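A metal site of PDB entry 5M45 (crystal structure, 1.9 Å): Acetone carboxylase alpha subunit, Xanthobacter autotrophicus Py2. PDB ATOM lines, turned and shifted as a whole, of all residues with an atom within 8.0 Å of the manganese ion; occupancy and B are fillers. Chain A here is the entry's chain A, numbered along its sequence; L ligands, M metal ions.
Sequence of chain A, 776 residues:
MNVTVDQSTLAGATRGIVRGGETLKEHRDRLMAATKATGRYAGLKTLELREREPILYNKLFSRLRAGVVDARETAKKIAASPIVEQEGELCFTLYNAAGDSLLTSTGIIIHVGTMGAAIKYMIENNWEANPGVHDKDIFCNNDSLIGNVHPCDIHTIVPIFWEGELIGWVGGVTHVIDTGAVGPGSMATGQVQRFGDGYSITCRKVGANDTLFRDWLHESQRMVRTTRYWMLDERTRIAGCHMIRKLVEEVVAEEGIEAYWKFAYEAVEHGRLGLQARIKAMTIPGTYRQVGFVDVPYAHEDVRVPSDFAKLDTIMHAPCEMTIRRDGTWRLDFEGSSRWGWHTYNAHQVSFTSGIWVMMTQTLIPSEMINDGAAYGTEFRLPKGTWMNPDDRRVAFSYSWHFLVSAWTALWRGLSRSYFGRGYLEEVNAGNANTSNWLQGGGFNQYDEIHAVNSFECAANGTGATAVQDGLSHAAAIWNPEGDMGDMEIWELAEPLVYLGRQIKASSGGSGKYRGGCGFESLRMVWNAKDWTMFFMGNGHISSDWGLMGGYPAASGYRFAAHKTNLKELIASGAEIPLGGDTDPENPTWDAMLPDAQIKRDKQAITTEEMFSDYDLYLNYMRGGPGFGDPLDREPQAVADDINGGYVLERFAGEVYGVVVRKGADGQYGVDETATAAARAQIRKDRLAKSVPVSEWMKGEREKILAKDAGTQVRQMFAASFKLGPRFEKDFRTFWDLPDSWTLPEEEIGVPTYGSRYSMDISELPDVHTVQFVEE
OD2 of Asp 153 sits close to NE2 of His 111, 2.8 Å away.
O of His 150 is in hydrogen-bond range of ND2 of Asn 148.
ND1 of His 150 sits at hydrogen-bond distance from O of Ser 398 (2.8 Å).
The backbone carbonyl oxygen (O) of Asp 153 lies within hydrogen-bond range of the side-chain amide nitrogen (ND2) of Asn 148.
NE2 of His 175 sits at hydrogen-bond distance from OG of Ser 186, 2.9 Å away.
O of Glu 89 lies within hydrogen-bond range of N of His 175 (3.3 Å).
The nearest printed residue that does not touch the manganese ion is Trp 401 (4.3 Å).
OD1 of Asp 153 is bound to the manganese ion, 2.1 Å away.
The manganese ion is bound by O1 of the ligand, at 2.2 Å.
O2 of the ligand is bound to the manganese ion, 2.3 Å away.
The manganese ion is bound by ND1 of His 175, 2.3 Å away.
The manganese ion is bound by NE2 of His 150 (2.3 Å).
The manganese ion is bound by OD2 of Asp 153.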
ATOM      1  N   ILE A  83     -18.096  15.248   2.412  1.00  0.00           N
ATOM      2  CA  ILE A  83     -16.880  15.958   2.847  1.00  0.00           C
ATOM      3  C   ILE A  83     -15.625  15.259   2.277  1.00  0.00           C
ATOM      4  O   ILE A  83     -14.717  15.924   1.755  1.00  0.00           O
ATOM      5  CB  ILE A  83     -16.830  16.095   4.373  1.00  0.00           C
ATOM      6  CG1 ILE A  83     -17.994  16.956   4.911  1.00  0.00           C
ATOM      7  CG2 ILE A  83     -15.490  16.688   4.839  1.00  0.00           C
ATOM      8  CD1 ILE A  83     -18.175  16.904   6.420  1.00  0.00           C
ATOM      9  N   GLU A  89     -11.723  16.289   1.209  1.00  0.00           N
ATOM     10  CA  GLU A  89     -11.048  16.702   2.470  1.00  0.00           C
ATOM     11  C   GLU A  89     -10.380  15.491   3.138  1.00  0.00           C
ATOM     12  O   GLU A  89     -10.835  14.981   4.171  1.00  0.00           O
ATOM     13  CB  GLU A  89     -11.987  17.470   3.418  1.00  0.00           C
ATOM     14  CG  GLU A  89     -12.875  18.554   2.770  1.00  0.00           C
ATOM     15  CD  GLU A  89     -12.160  19.567   1.891  1.00  0.00           C
ATOM     16  OE1 GLU A  89     -12.870  20.342   1.203  1.00  0.00           O
ATOM     17  OE2 GLU A  89     -10.895  19.637   1.878  1.00  0.00           O
ATOM     18  N   ILE A 108      -5.932  18.157   2.271  1.00  0.00           N
ATOM     19  CA  ILE A 108      -5.765  18.826   3.569  1.00  0.00           C
ATOM     20  C   ILE A 108      -4.362  18.613   4.135  1.00  0.00           C
ATOM     21  O   ILE A 108      -4.145  17.872   5.153  1.00  0.00           O
ATOM     22  CB  ILE A 108      -6.891  18.496   4.596  1.00  0.00           C
ATOM     23  CG1 ILE A 108      -7.187  16.977   4.717  1.00  0.00           C
ATOM     24  CG2 ILE A 108      -8.173  19.251   4.184  1.00  0.00           C
ATOM     25  CD1 ILE A 108      -8.071  16.623   5.900  1.00  0.00           C
ATOM     26  N   ILE A 110      -2.148  20.298   5.758  1.00  0.00           N
ATOM     27  CA  ILE A 110      -1.688  20.659   7.127  1.00  0.00           C
ATOM     28  C   ILE A 110      -1.312  19.394   7.903  1.00  0.00           C
ATOM     29  O   ILE A 110      -0.465  19.431   8.798  1.00  0.00           O
ATOM     30  CB  ILE A 110      -2.744  21.533   7.896  1.00  0.00           C
ATOM     31  CG1 ILE A 110      -2.088  22.258   9.085  1.00  0.00           C
ATOM     32  CG2 ILE A 110      -3.936  20.688   8.368  1.00  0.00           C
ATOM     33  CD1 ILE A 110      -2.940  23.383   9.640  1.00  0.00           C
ATOM     34  N   HIS A 111      -1.923  18.264   7.554  1.00  0.00           N
ATOM     35  CA  HIS A 111      -1.667  17.006   8.250  1.00  0.00           C
ATOM     36  C   HIS A 111      -0.382  16.297   7.867  1.00  0.00           C
ATOM     37  O   HIS A 111       0.008  15.321   8.521  1.00  0.00           O
ATOM     38  CB  HIS A 111      -2.897  16.089   8.156  1.00  0.00           C
ATOM     39  CG  HIS A 111      -4.107  16.706   8.783  1.00  0.00           C
ATOM     40  ND1 HIS A 111      -4.268  16.790  10.147  1.00  0.00           N
ATOM     41  CD2 HIS A 111      -5.170  17.346   8.244  1.00  0.00           C
ATOM     42  CE1 HIS A 111      -5.391  17.434  10.414  1.00  0.00           C
ATOM     43  NE2 HIS A 111      -5.958  17.777   9.282  1.00  0.00           N
ATOM     44  N   ASN A 148      -2.307  17.897  16.725  1.00  0.00           N
ATOM     45  CA  ASN A 148      -3.385  17.882  15.724  1.00  0.00           C
ATOM     46  C   ASN A 148      -4.229  19.204  15.712  1.00  0.00           C
ATOM     47  O   ASN A 148      -4.298  19.903  16.719  1.00  0.00           O
ATOM     48  CB  ASN A 148      -4.334  16.688  15.944  1.00  0.00           C
ATOM     49  CG  ASN A 148      -5.152  16.308  14.691  1.00  0.00           C
ATOM     50  OD1 ASN A 148      -4.782  16.663  13.554  1.00  0.00           O
ATOM     51  ND2 ASN A 148      -6.239  15.545  14.897  1.00  0.00           N
ATOM     52  N   VAL A 149      -4.907  19.467  14.586  1.00  0.00           N
ATOM     53  CA  VAL A 149      -5.762  20.625  14.433  1.00  0.00           C
ATOM     54  C   VAL A 149      -6.968  20.572  15.375  1.00  0.00           C
ATOM     55  O   VAL A 149      -7.209  21.512  16.148  1.00  0.00           O
ATOM     56  CB  VAL A 149      -6.256  20.745  12.961  1.00  0.00           C
ATOM     57  CG1 VAL A 149      -7.260  21.887  12.846  1.00  0.00           C
ATOM     58  CG2 VAL A 149      -5.094  20.946  12.010  1.00  0.00           C
ATOM     59  N   HIS A 150      -7.705  19.466  15.296  1.00  0.00           N
ATOM     60  CA  HIS A 150      -8.911  19.278  16.125  1.00  0.00           C
ATOM     61  C   HIS A 150      -9.337  17.812  16.092  1.00  0.00           C
ATOM     62  O   HIS A 150      -8.872  17.079  15.216  1.00  0.00           O
ATOM     63  CB  HIS A 150     -10.084  20.226  15.718  1.00  0.00           C
ATOM     64  CG  HIS A 150     -10.600  20.050  14.315  1.00  0.00           C
ATOM     65  ND1 HIS A 150     -11.754  20.661  13.889  1.00  0.00           N
ATOM     66  CD2 HIS A 150     -10.149  19.342  13.261  1.00  0.00           C
ATOM     67  CE1 HIS A 150     -11.949  20.395  12.608  1.00  0.00           C
ATOM     68  NE2 HIS A 150     -10.998  19.591  12.202  1.00  0.00           N
ATOM     69  N   PRO A 151     -10.198  17.389  17.027  1.00  0.00           N
ATOM     70  CA  PRO A 151     -10.584  15.962  17.065  1.00  0.00           C
ATOM     71  C   PRO A 151     -11.226  15.373  15.784  1.00  0.00           C
ATOM     72  O   PRO A 151     -10.984  14.208  15.478  1.00  0.00           O
ATOM     73  CB  PRO A 151     -11.526  15.881  18.263  1.00  0.00           C
ATOM     74  CG  PRO A 151     -11.056  17.011  19.170  1.00  0.00           C
ATOM     75  CD  PRO A 151     -10.711  18.122  18.211  1.00  0.00           C
ATOM     76  N   CYS A 152     -11.959  16.169  15.009  1.00  0.00           N
ATOM     77  CA  CYS A 152     -12.566  15.672  13.779  1.00  0.00           C
ATOM     78  C   CYS A 152     -11.610  15.259  12.631  1.00  0.00           C
ATOM     79  O   CYS A 152     -12.051  14.629  11.651  1.00  0.00           O
ATOM     80  CB  CYS A 152     -13.638  16.614  13.268  1.00  0.00           C
ATOM     81  SG  CYS A 152     -15.189  16.459  14.217  1.00  0.00           S
ATOM     82  N   ASP A 153     -10.316  15.624  12.711  1.00  0.00           N
ATOM     83  CA  ASP A 153      -9.342  15.132  11.762  1.00  0.00           C
ATOM     84  C   ASP A 153      -8.685  13.854  12.315  1.00  0.00           C
ATOM     85  O   ASP A 153      -7.785  13.925  13.158  1.00  0.00           O
ATOM     86  CB  ASP A 153      -8.327  16.198  11.409  1.00  0.00           C
ATOM     87  CG  ASP A 153      -8.931  17.334  10.617  1.00  0.00           C
ATOM     88  OD1 ASP A 153     -10.011  17.137   9.997  1.00  0.00           O
ATOM     89  OD2 ASP A 153      -8.366  18.458  10.614  1.00  0.00           O
ATOM     90  N   ILE A 154      -9.143  12.708  11.835  1.00  0.00           N
ATOM     91  CA  ILE A 154      -8.682  11.436  12.338  1.00  0.00           C
ATOM     92  C   ILE A 154      -7.534  10.890  11.474  1.00  0.00           C
ATOM     93  O   ILE A 154      -7.664  10.811  10.219  1.00  0.00           O
ATOM     94  CB  ILE A 154      -9.817  10.372  12.348  1.00  0.00           C
ATOM     95  CG1 ILE A 154     -11.092  10.904  13.053  1.00  0.00           C
ATOM     96  CG2 ILE A 154      -9.320   9.071  12.971  1.00  0.00           C
ATOM     97  CD1 ILE A 154     -10.921  11.189  14.531  1.00  0.00           C
ATOM     98  N   VAL A 173      -5.371  10.784   6.561  1.00  0.00           N
ATOM     99  CA  VAL A 173      -6.307  11.595   7.371  1.00  0.00           C
ATOM    100  C   VAL A 173      -7.612  11.832   6.620  1.00  0.00           C
ATOM    101  O   VAL A 173      -7.582  12.035   5.385  1.00  0.00           O
ATOM    102  CB  VAL A 173      -5.678  12.933   7.814  1.00  0.00           C
ATOM    103  CG1 VAL A 173      -5.230  13.768   6.598  1.00  0.00           C
ATOM    104  CG2 VAL A 173      -6.640  13.755   8.684  1.00  0.00           C
ATOM    105  N   THR A 174      -8.733  11.777   7.336  1.00  0.00           N
ATOM    106  CA  THR A 174     -10.035  12.251   6.832  1.00  0.00           C
ATOM    107  C   THR A 174     -10.664  13.198   7.861  1.00  0.00           C
ATOM    108  O   THR A 174     -10.646  12.898   9.073  1.00  0.00           O
ATOM    109  CB  THR A 174     -11.074  11.133   6.613  1.00  0.00           C
ATOM    110  OG1 THR A 174     -11.224  10.383   7.833  1.00  0.00           O
ATOM    111  CG2 THR A 174     -10.672  10.174   5.512  1.00  0.00           C
ATOM    112  N   HIS A 175     -11.243  14.301   7.406  1.00  0.00           N
ATOM    113  CA  HIS A 175     -12.143  15.091   8.255  1.00  0.00           C
ATOM    114  C   HIS A 175     -13.485  14.370   8.396  1.00  0.00           C
ATOM    115  O   HIS A 175     -14.173  14.196   7.386  1.00  0.00           O
ATOM    116  CB  HIS A 175     -12.390  16.497   7.675  1.00  0.00           C
ATOM    117  CG  HIS A 175     -13.380  17.291   8.490  1.00  0.00           C
ATOM    118  ND1 HIS A 175     -13.017  18.256   9.386  1.00  0.00           N
ATOM    119  CD2 HIS A 175     -14.729  17.148   8.618  1.00  0.00           C
ATOM    120  CE1 HIS A 175     -14.093  18.716  10.009  1.00  0.00           C
ATOM    121  NE2 HIS A 175     -15.145  18.057   9.558  1.00  0.00           N
ATOM    122  N   VAL A 176     -13.833  13.934   9.617  1.00  0.00           N
ATOM    123  CA  VAL A 176     -15.145  13.244   9.873  1.00  0.00           C
ATOM    124  C   VAL A 176     -16.210  14.244  10.328  1.00  0.00           C
ATOM    125  O   VAL A 176     -15.883  15.340  10.835  1.00  0.00           O
ATOM    126  CB  VAL A 176     -15.021  12.073  10.882  1.00  0.00           C
ATOM    127  CG1 VAL A 176     -13.923  11.099  10.428  1.00  0.00           C
ATOM    128  CG2 VAL A 176     -14.724  12.574  12.323  1.00  0.00           C
ATOM    129  N   SER A 186     -18.792  19.499  13.480  1.00  0.00           N
ATOM    130  CA  SER A 186     -17.325  19.346  13.505  1.00  0.00           C
ATOM    131  C   SER A 186     -16.638  20.500  14.228  1.00  0.00           C
ATOM    132  O   SER A 186     -15.674  20.293  14.956  1.00  0.00           O
ATOM    133  CB  SER A 186     -16.734  19.240  12.104  1.00  0.00           C
ATOM    134  OG  SER A 186     -17.458  18.407  11.203  1.00  0.00           O
ATOM    135  N   MET A 187     -17.147  21.722  14.012  1.00  0.00           N
ATOM    136  CA  MET A 187     -16.566  22.973  14.529  1.00  0.00           C
ATOM    137  C   MET A 187     -17.385  23.480  15.730  1.00  0.00           C
ATOM    138  O   MET A 187     -17.899  24.593  15.760  1.00  0.00           O
ATOM    139  CB  MET A 187     -16.585  24.035  13.416  1.00  0.00           C
ATOM    140  CG  MET A 187     -16.100  23.592  12.051  1.00  0.00           C
ATOM    141  SD  MET A 187     -14.497  22.713  12.029  1.00  0.00           S
ATOM    142  CE  MET A 187     -14.297  22.576  10.268  1.00  0.00           C
ATOM    143  N   SER A 398     -12.032  22.140  19.186  1.00  0.00           N
ATOM    144  CA  SER A 398     -12.930  21.710  18.053  1.00  0.00           C
ATOM    145  C   SER A 398     -12.949  22.671  16.866  1.00  0.00           C
ATOM    146  O   SER A 398     -13.138  22.220  15.741  1.00  0.00           O
ATOM    147  CB  SER A 398     -14.383  21.473  18.511  1.00  0.00           C
ATOM    148  OG  SER A 398     -14.524  20.233  19.207  1.00  0.00           O
ATOM    149  N   TRP A 401      -9.447  26.466  13.925  1.00  0.00           N
ATOM    150  CA  TRP A 401      -9.370  27.333  12.737  1.00  0.00           C
ATOM    151  C   TRP A 401      -9.764  28.777  12.981  1.00  0.00           C
ATOM    152  O   TRP A 401      -9.216  29.639  12.316  1.00  0.00           O
ATOM    153  CB  TRP A 401     -10.254  26.810  11.590  1.00  0.00           C
ATOM    154  CG  TRP A 401      -9.986  25.405  11.112  1.00  0.00           C
ATOM    155  CD1 TRP A 401     -10.834  24.345  11.172  1.00  0.00           C
ATOM    156  CD2 TRP A 401      -8.809  24.945  10.432  1.00  0.00           C
ATOM    157  NE1 TRP A 401     -10.277  23.247  10.540  1.00  0.00           N
ATOM    158  CE2 TRP A 401      -9.024  23.567  10.100  1.00  0.00           C
ATOM    159  CE3 TRP A 401      -7.588  25.539  10.068  1.00  0.00           C
ATOM    160  CZ2 TRP A 401      -8.070  22.812   9.445  1.00  0.00           C
ATOM    161  CZ3 TRP A 401      -6.648  24.763   9.388  1.00  0.00           C
ATOM    162  CH2 TRP A 401      -6.894  23.417   9.086  1.00  0.00           C
ATOM    163  N   TRP A 438     -19.788  28.058   9.315  1.00  0.00           N
ATOM    164  CA  TRP A 438     -19.981  26.611   9.378  1.00  0.00           C
ATOM    165  C   TRP A 438     -21.420  26.254   9.859  1.00  0.00           C
ATOM    166  O   TRP A 438     -21.755  26.385  11.061  1.00  0.00           O
ATOM    167  CB  TRP A 438     -18.930  25.969  10.308  1.00  0.00           C
ATOM    168  CG  TRP A 438     -17.525  26.145   9.856  1.00  0.00           C
ATOM    169  CD1 TRP A 438     -16.656  27.141  10.238  1.00  0.00           C
ATOM    170  CD2 TRP A 438     -16.795  25.319   8.917  1.00  0.00           C
ATOM    171  NE1 TRP A 438     -15.449  27.003   9.614  1.00  0.00           N
ATOM    172  CE2 TRP A 438     -15.498  25.910   8.778  1.00  0.00           C
ATOM    173  CE3 TRP A 438     -17.109  24.192   8.168  1.00  0.00           C
ATOM    174  CZ2 TRP A 438     -14.512  25.373   7.933  1.00  0.00           C
ATOM    175  CZ3 TRP A 438     -16.122  23.637   7.310  1.00  0.00           C
ATOM    176  CH2 TRP A 438     -14.811  24.236   7.230  1.00  0.00           C
ATOM    177  N   ASN A 454     -22.485  19.305   9.076  1.00  0.00           N
ATOM    178  CA  ASN A 454     -21.381  20.242   9.081  1.00  0.00           C
ATOM    179  C   ASN A 454     -21.047  20.593   7.629  1.00  0.00           C
ATOM    180  O   ASN A 454     -20.249  19.897   6.991  1.00  0.00           O
ATOM    181  CB  ASN A 454     -20.157  19.661   9.794  1.00  0.00           C
ATOM    182  CG  ASN A 454     -19.084  20.731  10.059  1.00  0.00           C
ATOM    183  OD1 ASN A 454     -18.975  21.260  11.155  1.00  0.00           O
ATOM    184  ND2 ASN A 454     -18.269  21.033   9.046  1.00  0.00           N
ATOM    185  N   PHE A 456     -19.576  21.935   4.267  1.00  0.00           N
ATOM    186  CA  PHE A 456     -18.304  22.409   3.695  1.00  0.00           C
ATOM    187  C   PHE A 456     -18.497  23.385   2.494  1.00  0.00           C
ATOM    188  O   PHE A 456     -17.599  23.540   1.662  1.00  0.00           O
ATOM    189  CB  PHE A 456     -17.354  21.222   3.366  1.00  0.00           C
ATOM    190  CG  PHE A 456     -16.387  20.889   4.491  1.00  0.00           C
ATOM    191  CD1 PHE A 456     -16.825  20.280   5.649  1.00  0.00           C
ATOM    192  CD2 PHE A 456     -15.016  21.161   4.358  1.00  0.00           C
ATOM    193  CE1 PHE A 456     -15.946  19.986   6.683  1.00  0.00           C
ATOM    194  CE2 PHE A 456     -14.150  20.892   5.371  1.00  0.00           C
ATOM    195  CZ  PHE A 456     -14.594  20.278   6.537  1.00  0.00           C
ATOM    196  N   TRP A 479      -6.773  26.366   4.067  1.00  0.00           N
ATOM    197  CA  TRP A 479      -6.452  24.960   4.371  1.00  0.00           C
ATOM    198  C   TRP A 479      -6.633  23.970   3.187  1.00  0.00           C
ATOM    199  O   TRP A 479      -6.329  22.771   3.329  1.00  0.00           O
ATOM    200  CB  TRP A 479      -7.203  24.448   5.648  1.00  0.00           C
ATOM    201  CG  TRP A 479      -8.603  24.940   5.804  1.00  0.00           C
ATOM    202  CD1 TRP A 479      -9.025  25.945   6.638  1.00  0.00           C
ATOM    203  CD2 TRP A 479      -9.763  24.517   5.090  1.00  0.00           C
ATOM    204  NE1 TRP A 479     -10.359  26.156   6.506  1.00  0.00           N
ATOM    205  CE2 TRP A 479     -10.858  25.283   5.566  1.00  0.00           C
ATOM    206  CE3 TRP A 479      -9.996  23.524   4.124  1.00  0.00           C
ATOM    207  CZ2 TRP A 479     -12.152  25.130   5.082  1.00  0.00           C
ATOM    208  CZ3 TRP A 479     -11.286  23.363   3.637  1.00  0.00           C
ATOM    209  CH2 TRP A 479     -12.349  24.161   4.131  1.00  0.00           C
HETATM  210  C1  LIG L   1     -10.885  20.880   8.226  1.00  0.00           C
HETATM  211  O1  LIG L   1     -11.318  21.027   9.384  1.00  0.00           O
HETATM  212  O2  LIG L   1     -10.369  19.795   7.875  1.00  0.00           O
HETATM  213  C2  LIG L   1     -10.997  22.012   7.241  1.00  0.00           C
HETATM  214 MN    MN M   1     -10.908  18.984   9.960  1.00  0.00          MN
